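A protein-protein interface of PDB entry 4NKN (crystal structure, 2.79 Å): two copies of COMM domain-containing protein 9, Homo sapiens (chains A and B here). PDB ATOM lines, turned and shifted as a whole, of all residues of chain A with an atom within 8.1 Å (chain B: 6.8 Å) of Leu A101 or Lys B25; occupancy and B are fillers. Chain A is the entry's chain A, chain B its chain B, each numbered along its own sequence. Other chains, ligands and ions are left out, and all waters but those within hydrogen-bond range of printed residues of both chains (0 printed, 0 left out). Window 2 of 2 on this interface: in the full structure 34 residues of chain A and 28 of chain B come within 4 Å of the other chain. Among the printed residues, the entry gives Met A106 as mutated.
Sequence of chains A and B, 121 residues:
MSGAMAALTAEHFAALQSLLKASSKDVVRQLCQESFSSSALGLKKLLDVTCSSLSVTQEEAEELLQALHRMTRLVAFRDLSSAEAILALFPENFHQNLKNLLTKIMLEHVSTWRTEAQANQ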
ATOM      1  N   LEU A  87      20.296 -13.263  20.200  1.00  0.00           N
ATOM      2  CA  LEU A  87      21.448 -14.048  19.760  1.00  0.00           C
ATOM      3  C   LEU A  87      21.010 -15.397  19.200  1.00  0.00           C
ATOM      4  O   LEU A  87      21.723 -16.012  18.405  1.00  0.00           O
ATOM      5  CB  LEU A  87      22.435 -14.259  20.911  1.00  0.00           C
ATOM      6  CG  LEU A  87      23.334 -13.087  21.312  1.00  0.00           C
ATOM      7  CD1 LEU A  87      24.092 -13.413  22.589  1.00  0.00           C
ATOM      8  CD2 LEU A  87      24.302 -12.746  20.193  1.00  0.00           C
ATOM      9  N   PHE A  90      20.628 -15.677  15.216  1.00  0.00           N
ATOM     10  CA  PHE A  90      21.784 -15.820  14.337  1.00  0.00           C
ATOM     11  C   PHE A  90      22.301 -17.255  14.279  1.00  0.00           C
ATOM     12  O   PHE A  90      22.372 -17.937  15.302  1.00  0.00           O
ATOM     13  CB  PHE A  90      22.913 -14.887  14.786  1.00  0.00           C
ATOM     14  CG  PHE A  90      22.565 -13.430  14.705  1.00  0.00           C
ATOM     15  CD1 PHE A  90      22.896 -12.685  13.586  1.00  0.00           C
ATOM     16  CD2 PHE A  90      21.906 -12.804  15.751  1.00  0.00           C
ATOM     17  CE1 PHE A  90      22.578 -11.344  13.509  1.00  0.00           C
ATOM     18  CE2 PHE A  90      21.584 -11.462  15.680  1.00  0.00           C
ATOM     19  CZ  PHE A  90      21.921 -10.731  14.558  1.00  0.00           C
ATOM     20  N   PHE A  94      27.710 -17.464  11.650  1.00  0.00           N
ATOM     21  CA  PHE A  94      27.629 -16.017  11.486  1.00  0.00           C
ATOM     22  C   PHE A  94      28.769 -15.331  12.233  1.00  0.00           C
ATOM     23  O   PHE A  94      29.183 -15.787  13.300  1.00  0.00           O
ATOM     24  CB  PHE A  94      26.275 -15.497  11.977  1.00  0.00           C
ATOM     25  CG  PHE A  94      25.962 -14.097  11.526  1.00  0.00           C
ATOM     26  CD1 PHE A  94      25.310 -13.871  10.323  1.00  0.00           C
ATOM     27  CD2 PHE A  94      26.313 -13.007  12.307  1.00  0.00           C
ATOM     28  CE1 PHE A  94      25.017 -12.584   9.908  1.00  0.00           C
ATOM     29  CE2 PHE A  94      26.023 -11.720  11.896  1.00  0.00           C
ATOM     30  CZ  PHE A  94      25.374 -11.507  10.696  1.00  0.00           C
ATOM     31  N   HIS A  95      29.273 -14.241  11.657  1.00  0.00           N
ATOM     32  CA  HIS A  95      30.389 -13.491  12.229  1.00  0.00           C
ATOM     33  C   HIS A  95      30.090 -13.075  13.666  1.00  0.00           C
ATOM     34  O   HIS A  95      29.118 -12.367  13.925  1.00  0.00           O
ATOM     35  CB  HIS A  95      30.695 -12.262  11.371  1.00  0.00           C
ATOM     36  CG  HIS A  95      31.995 -11.600  11.701  1.00  0.00           C
ATOM     37  ND1 HIS A  95      32.106 -10.605  12.648  1.00  0.00           N
ATOM     38  CD2 HIS A  95      33.240 -11.783  11.202  1.00  0.00           C
ATOM     39  CE1 HIS A  95      33.363 -10.207  12.722  1.00  0.00           C
ATOM     40  NE2 HIS A  95      34.072 -10.906  11.854  1.00  0.00           N
ATOM     41  N   GLN A  96      30.934 -13.523  14.590  1.00  0.00           N
ATOM     42  CA  GLN A  96      30.702 -13.348  16.023  1.00  0.00           C
ATOM     43  C   GLN A  96      30.609 -11.886  16.454  1.00  0.00           C
ATOM     44  O   GLN A  96      29.685 -11.504  17.174  1.00  0.00           O
ATOM     45  CB  GLN A  96      31.804 -14.046  16.822  1.00  0.00           C
ATOM     46  N   ASN A  97      31.570 -11.074  16.021  1.00  0.00           N
ATOM     47  CA  ASN A  97      31.608  -9.664  16.402  1.00  0.00           C
ATOM     48  C   ASN A  97      30.417  -8.873  15.871  1.00  0.00           C
ATOM     49  O   ASN A  97      29.878  -8.014  16.566  1.00  0.00           O
ATOM     50  CB  ASN A  97      32.910  -9.017  15.924  1.00  0.00           C
ATOM     51  CG  ASN A  97      34.088  -9.355  16.815  1.00  0.00           C
ATOM     52  OD1 ASN A  97      33.915  -9.819  17.943  1.00  0.00           O
ATOM     53  ND2 ASN A  97      35.295  -9.110  16.319  1.00  0.00           N
ATOM     54  N   LEU A  98      30.013  -9.159  14.637  1.00  0.00           N
ATOM     55  CA  LEU A  98      28.844  -8.511  14.057  1.00  0.00           C
ATOM     56  C   LEU A  98      27.577  -9.020  14.732  1.00  0.00           C
ATOM     57  O   LEU A  98      26.607  -8.281  14.898  1.00  0.00           O
ATOM     58  CB  LEU A  98      28.780  -8.753  12.547  1.00  0.00           C
ATOM     59  CG  LEU A  98      27.580  -8.148  11.816  1.00  0.00           C
ATOM     60  CD1 LEU A  98      27.483  -6.654  12.083  1.00  0.00           C
ATOM     61  CD2 LEU A  98      27.671  -8.424  10.323  1.00  0.00           C
ATOM     62  N   LYS A  99      27.596 -10.291  15.119  1.00  0.00           N
ATOM     63  CA  LYS A  99      26.484 -10.895  15.840  1.00  0.00           C
ATOM     64  C   LYS A  99      26.264 -10.191  17.175  1.00  0.00           C
ATOM     65  O   LYS A  99      25.127  -9.979  17.600  1.00  0.00           O
ATOM     66  CB  LYS A  99      26.743 -12.385  16.059  1.00  0.00           C
ATOM     67  CG  LYS A  99      25.644 -13.125  16.792  1.00  0.00           C
ATOM     68  CD  LYS A  99      26.026 -14.584  16.988  1.00  0.00           C
ATOM     69  CE  LYS A  99      24.948 -15.352  17.735  1.00  0.00           C
ATOM     70  NZ  LYS A  99      25.316 -16.780  17.947  1.00  0.00           N
ATOM     71  N   ASN A 100      27.365  -9.828  17.827  1.00  0.00           N
ATOM     72  CA  ASN A 100      27.312  -9.124  19.105  1.00  0.00           C
ATOM     73  C   ASN A 100      26.946  -7.655  18.945  1.00  0.00           C
ATOM     74  O   ASN A 100      26.238  -7.091  19.779  1.00  0.00           O
ATOM     75  CB  ASN A 100      28.650  -9.235  19.832  1.00  0.00           C
ATOM     76  CG  ASN A 100      28.999 -10.661  20.199  1.00  0.00           C
ATOM     77  OD1 ASN A 100      28.119 -11.502  20.384  1.00  0.00           O
ATOM     78  ND2 ASN A 100      30.292 -10.942  20.311  1.00  0.00           N
ATOM     79  N   LEU A 101      27.437  -7.032  17.880  1.00  0.00           N
ATOM     80  CA  LEU A 101      27.153  -5.623  17.641  1.00  0.00           C
ATOM     81  C   LEU A 101      25.674  -5.427  17.333  1.00  0.00           C
ATOM     82  O   LEU A 101      25.028  -4.540  17.890  1.00  0.00           O
ATOM     83  CB  LEU A 101      28.009  -5.077  16.497  1.00  0.00           C
ATOM     84  CG  LEU A 101      27.830  -3.589  16.191  1.00  0.00           C
ATOM     85  CD1 LEU A 101      28.131  -2.746  17.425  1.00  0.00           C
ATOM     86  CD2 LEU A 101      28.703  -3.162  15.018  1.00  0.00           C
ATOM     87  N   LEU A 102      25.139  -6.273  16.458  1.00  0.00           N
ATOM     88  CA  LEU A 102      23.741  -6.180  16.056  1.00  0.00           C
ATOM     89  C   LEU A 102      22.785  -6.480  17.209  1.00  0.00           C
ATOM     90  O   LEU A 102      21.765  -5.808  17.361  1.00  0.00           O
ATOM     91  CB  LEU A 102      23.461  -7.125  14.885  1.00  0.00           C
ATOM     92  CG  LEU A 102      24.023  -6.680  13.533  1.00  0.00           C
ATOM     93  CD1 LEU A 102      23.771  -7.728  12.460  1.00  0.00           C
ATOM     94  CD2 LEU A 102      23.416  -5.349  13.135  1.00  0.00           C
ATOM     95  N   THR A 103      23.113  -7.478  18.024  1.00  0.00           N
ATOM     96  CA  THR A 103      22.251  -7.842  19.145  1.00  0.00           C
ATOM     97  C   THR A 103      22.299  -6.784  20.246  1.00  0.00           C
ATOM     98  O   THR A 103      21.386  -6.694  21.066  1.00  0.00           O
ATOM     99  CB  THR A 103      22.628  -9.213  19.742  1.00  0.00           C
ATOM    100  OG1 THR A 103      21.593  -9.647  20.633  1.00  0.00           O
ATOM    101  CG2 THR A 103      23.936  -9.127  20.504  1.00  0.00           C
ATOM    102  N   LYS A 104      23.366  -5.990  20.263  1.00  0.00           N
ATOM    103  CA  LYS A 104      23.484  -4.883  21.206  1.00  0.00           C
ATOM    104  C   LYS A 104      22.641  -3.702  20.742  1.00  0.00           C
ATOM    105  O   LYS A 104      21.899  -3.111  21.526  1.00  0.00           O
ATOM    106  CB  LYS A 104      24.945  -4.454  21.367  1.00  0.00           C
ATOM    107  CG  LYS A 104      25.741  -5.280  22.361  1.00  0.00           C
ATOM    108  CD  LYS A 104      27.165  -4.761  22.485  1.00  0.00           C
ATOM    109  CE  LYS A 104      27.933  -5.490  23.578  1.00  0.00           C
ATOM    110  NZ  LYS A 104      28.003  -6.958  23.335  1.00  0.00           N
ATOM    111  N   ILE A 105      22.764  -3.370  19.462  1.00  0.00           N
ATOM    112  CA  ILE A 105      22.038  -2.253  18.866  1.00  0.00           C
ATOM    113  C   ILE A 105      20.525  -2.429  18.977  1.00  0.00           C
ATOM    114  O   ILE A 105      19.799  -1.482  19.277  1.00  0.00           O
ATOM    115  CB  ILE A 105      22.422  -2.074  17.380  1.00  0.00           C
ATOM    116  CG1 ILE A 105      23.893  -1.671  17.256  1.00  0.00           C
ATOM    117  CG2 ILE A 105      21.538  -1.035  16.713  1.00  0.00           C
ATOM    118  CD1 ILE A 105      24.378  -1.552  15.826  1.00  0.00           C
ATOM    119  N   MET A 106      20.055  -3.652  18.756  1.00  0.00           N
ATOM    120  CA  MET A 106      18.623  -3.926  18.764  1.00  0.00           C
ATOM    121  C   MET A 106      18.073  -4.204  20.162  1.00  0.00           C
ATOM    122  O   MET A 106      16.860  -4.247  20.355  1.00  0.00           O
ATOM    123  CB  MET A 106      18.311  -5.103  17.839  1.00  0.00           C
ATOM    124  CG  MET A 106      18.665  -4.837  16.387  1.00  0.00           C
ATOM    125  SD  MET A 106      18.299  -6.354  15.232  1.00  0.00           S
ATOM    126  CE  MET A 106      19.482  -7.675  16.040  1.00  0.00           C
ATOM    127  N   LEU A 107      18.961  -4.400  21.131  1.00  0.00           N
ATOM    128  CA  LEU A 107      18.534  -4.570  22.514  1.00  0.00           C
ATOM    129  C   LEU A 107      18.290  -3.199  23.140  1.00  0.00           C
ATOM    130  O   LEU A 107      17.586  -3.074  24.145  1.00  0.00           O
ATOM    131  CB  LEU A 107      19.574  -5.355  23.316  1.00  0.00           C
ATOM    132  CG  LEU A 107      19.171  -5.828  24.714  1.00  0.00           C
ATOM    133  CD1 LEU A 107      17.858  -6.594  24.661  1.00  0.00           C
ATOM    134  CD2 LEU A 107      20.267  -6.682  25.339  1.00  0.00           C
ATOM    135  N   GLU A 108      18.876  -2.173  22.529  1.00  0.00           N
ATOM    136  CA  GLU A 108      18.687  -0.797  22.970  1.00  0.00           C
ATOM    137  C   GLU A 108      17.373  -0.226  22.453  1.00  0.00           C
ATOM    138  O   GLU A 108      16.666   0.485  23.168  1.00  0.00           O
ATOM    139  CB  GLU A 108      19.843   0.087  22.495  1.00  0.00           C
ATOM    140  CG  GLU A 108      21.221  -0.350  22.954  1.00  0.00           C
ATOM    141  CD  GLU A 108      22.323   0.519  22.375  1.00  0.00           C
ATOM    142  OE1 GLU A 108      22.035   1.677  22.000  1.00  0.00           O
ATOM    143  OE2 GLU A 108      23.474   0.042  22.287  1.00  0.00           O
ATOM    144  N   LEU B  19      27.540  -5.461   6.571  1.00  0.00           N
ATOM    145  CA  LEU B  19      27.777  -4.429   7.578  1.00  0.00           C
ATOM    146  C   LEU B  19      29.224  -4.422   8.063  1.00  0.00           C
ATOM    147  O   LEU B  19      29.660  -3.481   8.727  1.00  0.00           O
ATOM    148  CB  LEU B  19      26.830  -4.621   8.767  1.00  0.00           C
ATOM    149  CG  LEU B  19      25.343  -4.382   8.500  1.00  0.00           C
ATOM    150  CD1 LEU B  19      24.503  -4.876   9.665  1.00  0.00           C
ATOM    151  CD2 LEU B  19      25.071  -2.911   8.234  1.00  0.00           C
ATOM    152  N   ALA B  22      31.401  -1.522   6.811  1.00  0.00           N
ATOM    153  CA  ALA B  22      31.174  -0.187   7.354  1.00  0.00           C
ATOM    154  C   ALA B  22      32.439   0.394   7.974  1.00  0.00           C
ATOM    155  O   ALA B  22      33.311  -0.340   8.438  1.00  0.00           O
ATOM    156  CB  ALA B  22      30.052  -0.220   8.379  1.00  0.00           C
ATOM    157  N   SER B  23      32.526   1.721   7.976  1.00  0.00           N
ATOM    158  CA  SER B  23      33.698   2.417   8.498  1.00  0.00           C
ATOM    159  C   SER B  23      33.692   2.490  10.025  1.00  0.00           C
ATOM    160  O   SER B  23      34.750   2.491  10.655  1.00  0.00           O
ATOM    161  CB  SER B  23      33.783   3.827   7.910  1.00  0.00           C
ATOM    162  OG  SER B  23      32.625   4.582   8.226  1.00  0.00           O
ATOM    163  N   SER B  24      32.502   2.553  10.614  1.00  0.00           N
ATOM    164  CA  SER B  24      32.377   2.624  12.067  1.00  0.00           C
ATOM    165  C   SER B  24      31.097   1.956  12.556  1.00  0.00           C
ATOM    166  O   SER B  24      30.219   1.616  11.763  1.00  0.00           O
ATOM    167  CB  SER B  24      32.414   4.079  12.541  1.00  0.00           C
ATOM    168  OG  SER B  24      31.253   4.781  12.130  1.00  0.00           O
ATOM    169  N   LYS B  25      30.998   1.780  13.869  1.00  0.00           N
ATOM    170  CA  LYS B  25      29.839   1.134  14.475  1.00  0.00           C
ATOM    171  C   LYS B  25      28.619   2.048  14.463  1.00  0.00           C
ATOM    172  O   LYS B  25      27.492   1.594  14.660  1.00  0.00           O
ATOM    173  CB  LYS B  25      30.155   0.706  15.909  1.00  0.00           C
ATOM    174  CG  LYS B  25      31.267  -0.325  16.031  1.00  0.00           C
ATOM    175  CD  LYS B  25      31.460  -0.741  17.481  1.00  0.00           C
ATOM    176  CE  LYS B  25      32.588  -1.748  17.637  1.00  0.00           C
ATOM    177  NZ  LYS B  25      32.756  -2.163  19.059  1.00  0.00           N
ATOM    178  N   ASP B  26      28.850   3.337  14.237  1.00  0.00           N
ATOM    179  CA  ASP B  26      27.764   4.308  14.225  1.00  0.00           C
ATOM    180  C   ASP B  26      26.947   4.185  12.944  1.00  0.00           C
ATOM    181  O   ASP B  26      25.734   4.394  12.950  1.00  0.00           O
ATOM    182  CB  ASP B  26      28.309   5.730  14.375  1.00  0.00           C
ATOM    183  CG  ASP B  26      27.248   6.715  14.836  1.00  0.00           C
ATOM    184  OD1 ASP B  26      26.256   6.275  15.454  1.00  0.00           O
ATOM    185  OD2 ASP B  26      27.410   7.929  14.589  1.00  0.00           O
ATOM    186  N   VAL B  27      27.618   3.843  11.849  1.00  0.00           N
ATOM    187  CA  VAL B  27      26.945   3.634  10.571  1.00  0.00           C
ATOM    188  C   VAL B  27      26.015   2.430  10.655  1.00  0.00           C
ATOM    189  O   VAL B  27      24.880   2.467  10.179  1.00  0.00           O
ATOM    190  CB  VAL B  27      27.948   3.419   9.425  1.00  0.00           C
ATOM    191  CG1 VAL B  27      27.214   3.270   8.103  1.00  0.00           C
ATOM    192  CG2 VAL B  27      28.943   4.568   9.363  1.00  0.00           C
ATOM    193  N   VAL B  28      26.516   1.364  11.271  1.00  0.00           N
ATOM    194  CA  VAL B  28      25.737   0.156  11.502  1.00  0.00           C
ATOM    195  C   VAL B  28      24.508   0.470  12.353  1.00  0.00           C
ATOM    196  O   VAL B  28      23.423  -0.060  12.117  1.00  0.00           O
ATOM    197  CB  VAL B  28      26.587  -0.926  12.194  1.00  0.00           C
ATOM    198  CG1 VAL B  28      25.770  -2.184  12.432  1.00  0.00           C
ATOM    199  CG2 VAL B  28      27.827  -1.234  11.364  1.00  0.00           C
ATOM    200  N   ARG B  29      24.690   1.348  13.334  1.00  0.00           N
ATOM    201  CA  ARG B  29      23.602   1.751  14.218  1.00  0.00           C
ATOM    202  C   ARG B  29      22.557   2.575  13.470  1.00  0.00           C
ATOM    203  O   ARG B  29      21.356   2.413  13.689  1.00  0.00           O
ATOM    204  CB  ARG B  29      24.149   2.547  15.405  1.00  0.00           C
ATOM    205  CG  ARG B  29      23.162   2.723  16.546  1.00  0.00           C
ATOM    206  CD  ARG B  29      23.787   3.502  17.691  1.00  0.00           C
ATOM    207  NE  ARG B  29      25.124   3.009  18.012  1.00  0.00           N
ATOM    208  CZ  ARG B  29      25.375   2.021  18.864  1.00  0.00           C
ATOM    209  NH1 ARG B  29      24.378   1.409  19.490  1.00  0.00           N
ATOM    210  NH2 ARG B  29      26.626   1.643  19.091  1.00  0.00           N
ATOM    211  N   GLN B  30      23.021   3.457  12.592  1.00  0.00           N
ATOM    212  CA  GLN B  30      22.126   4.305  11.812  1.00  0.00           C
ATOM    213  C   GLN B  30      21.291   3.484  10.837  1.00  0.00           C
ATOM    214  O   GLN B  30      20.082   3.687  10.717  1.00  0.00           O
ATOM    215  CB  GLN B  30      22.916   5.364  11.044  1.00  0.00           C
ATOM    216  CG  GLN B  30      22.054   6.233  10.141  1.00  0.00           C
ATOM    217  CD  GLN B  30      22.863   6.989   9.106  1.00  0.00           C
ATOM    218  OE1 GLN B  30      24.073   6.796   8.984  1.00  0.00           O
ATOM    219  NE2 GLN B  30      22.197   7.855   8.351  1.00  0.00           N
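No position is printed for both chains. Of the 6 pairs that touch across the chains among the printed residues, none has its exchanged pair printed and touching as well.
ND1 of His A95 lies within hydrogen-bond range of N of Leu A98 (3.2 Å).
Leu B19 touches Leu A98. Leu A101 touches Lys B25 (CD1 to CD, 3.9 Å). Leu B19 touches Leu A102. Ile A105 touches Val B28. Arg B29 touches Ile A105 (CA to CD1, 3.8 Å).
Of chain B, only Lys B25 comes within 4 Å of Leu A101. Lys B25 touches just one residue of chain A: Leu A101 (3.9 Å). No residue of chain A comes within 4 Å of Ser B24. Of the printed residues of chain B, Glu A108 touches Arg B29. Of the printed residues of chain B, Leu A102 touches Leu B19. The nearest residue of chain B that does not touch Leu A101 is Val B28 (4.03 Å). The nearest residue of chain A that does not touch Lys B25 is Ile A105 (4.6 Å). The nearest printed residue of chain B that does not touch Ile A105 is Lys B25 (4.6 Å).
Hydrophobic or aromatic side chains of chain B that line the printed part of chain A: Leu B19 and Val B28. Printed residues of chain A that touch a printed residue of chain B: Leu A98, Leu A101, Leu A102, Ile A105 and Glu A108.
NH1 of Arg B29 is in salt-bridge range of OE2 of Glu A108, at 3.2 Å.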
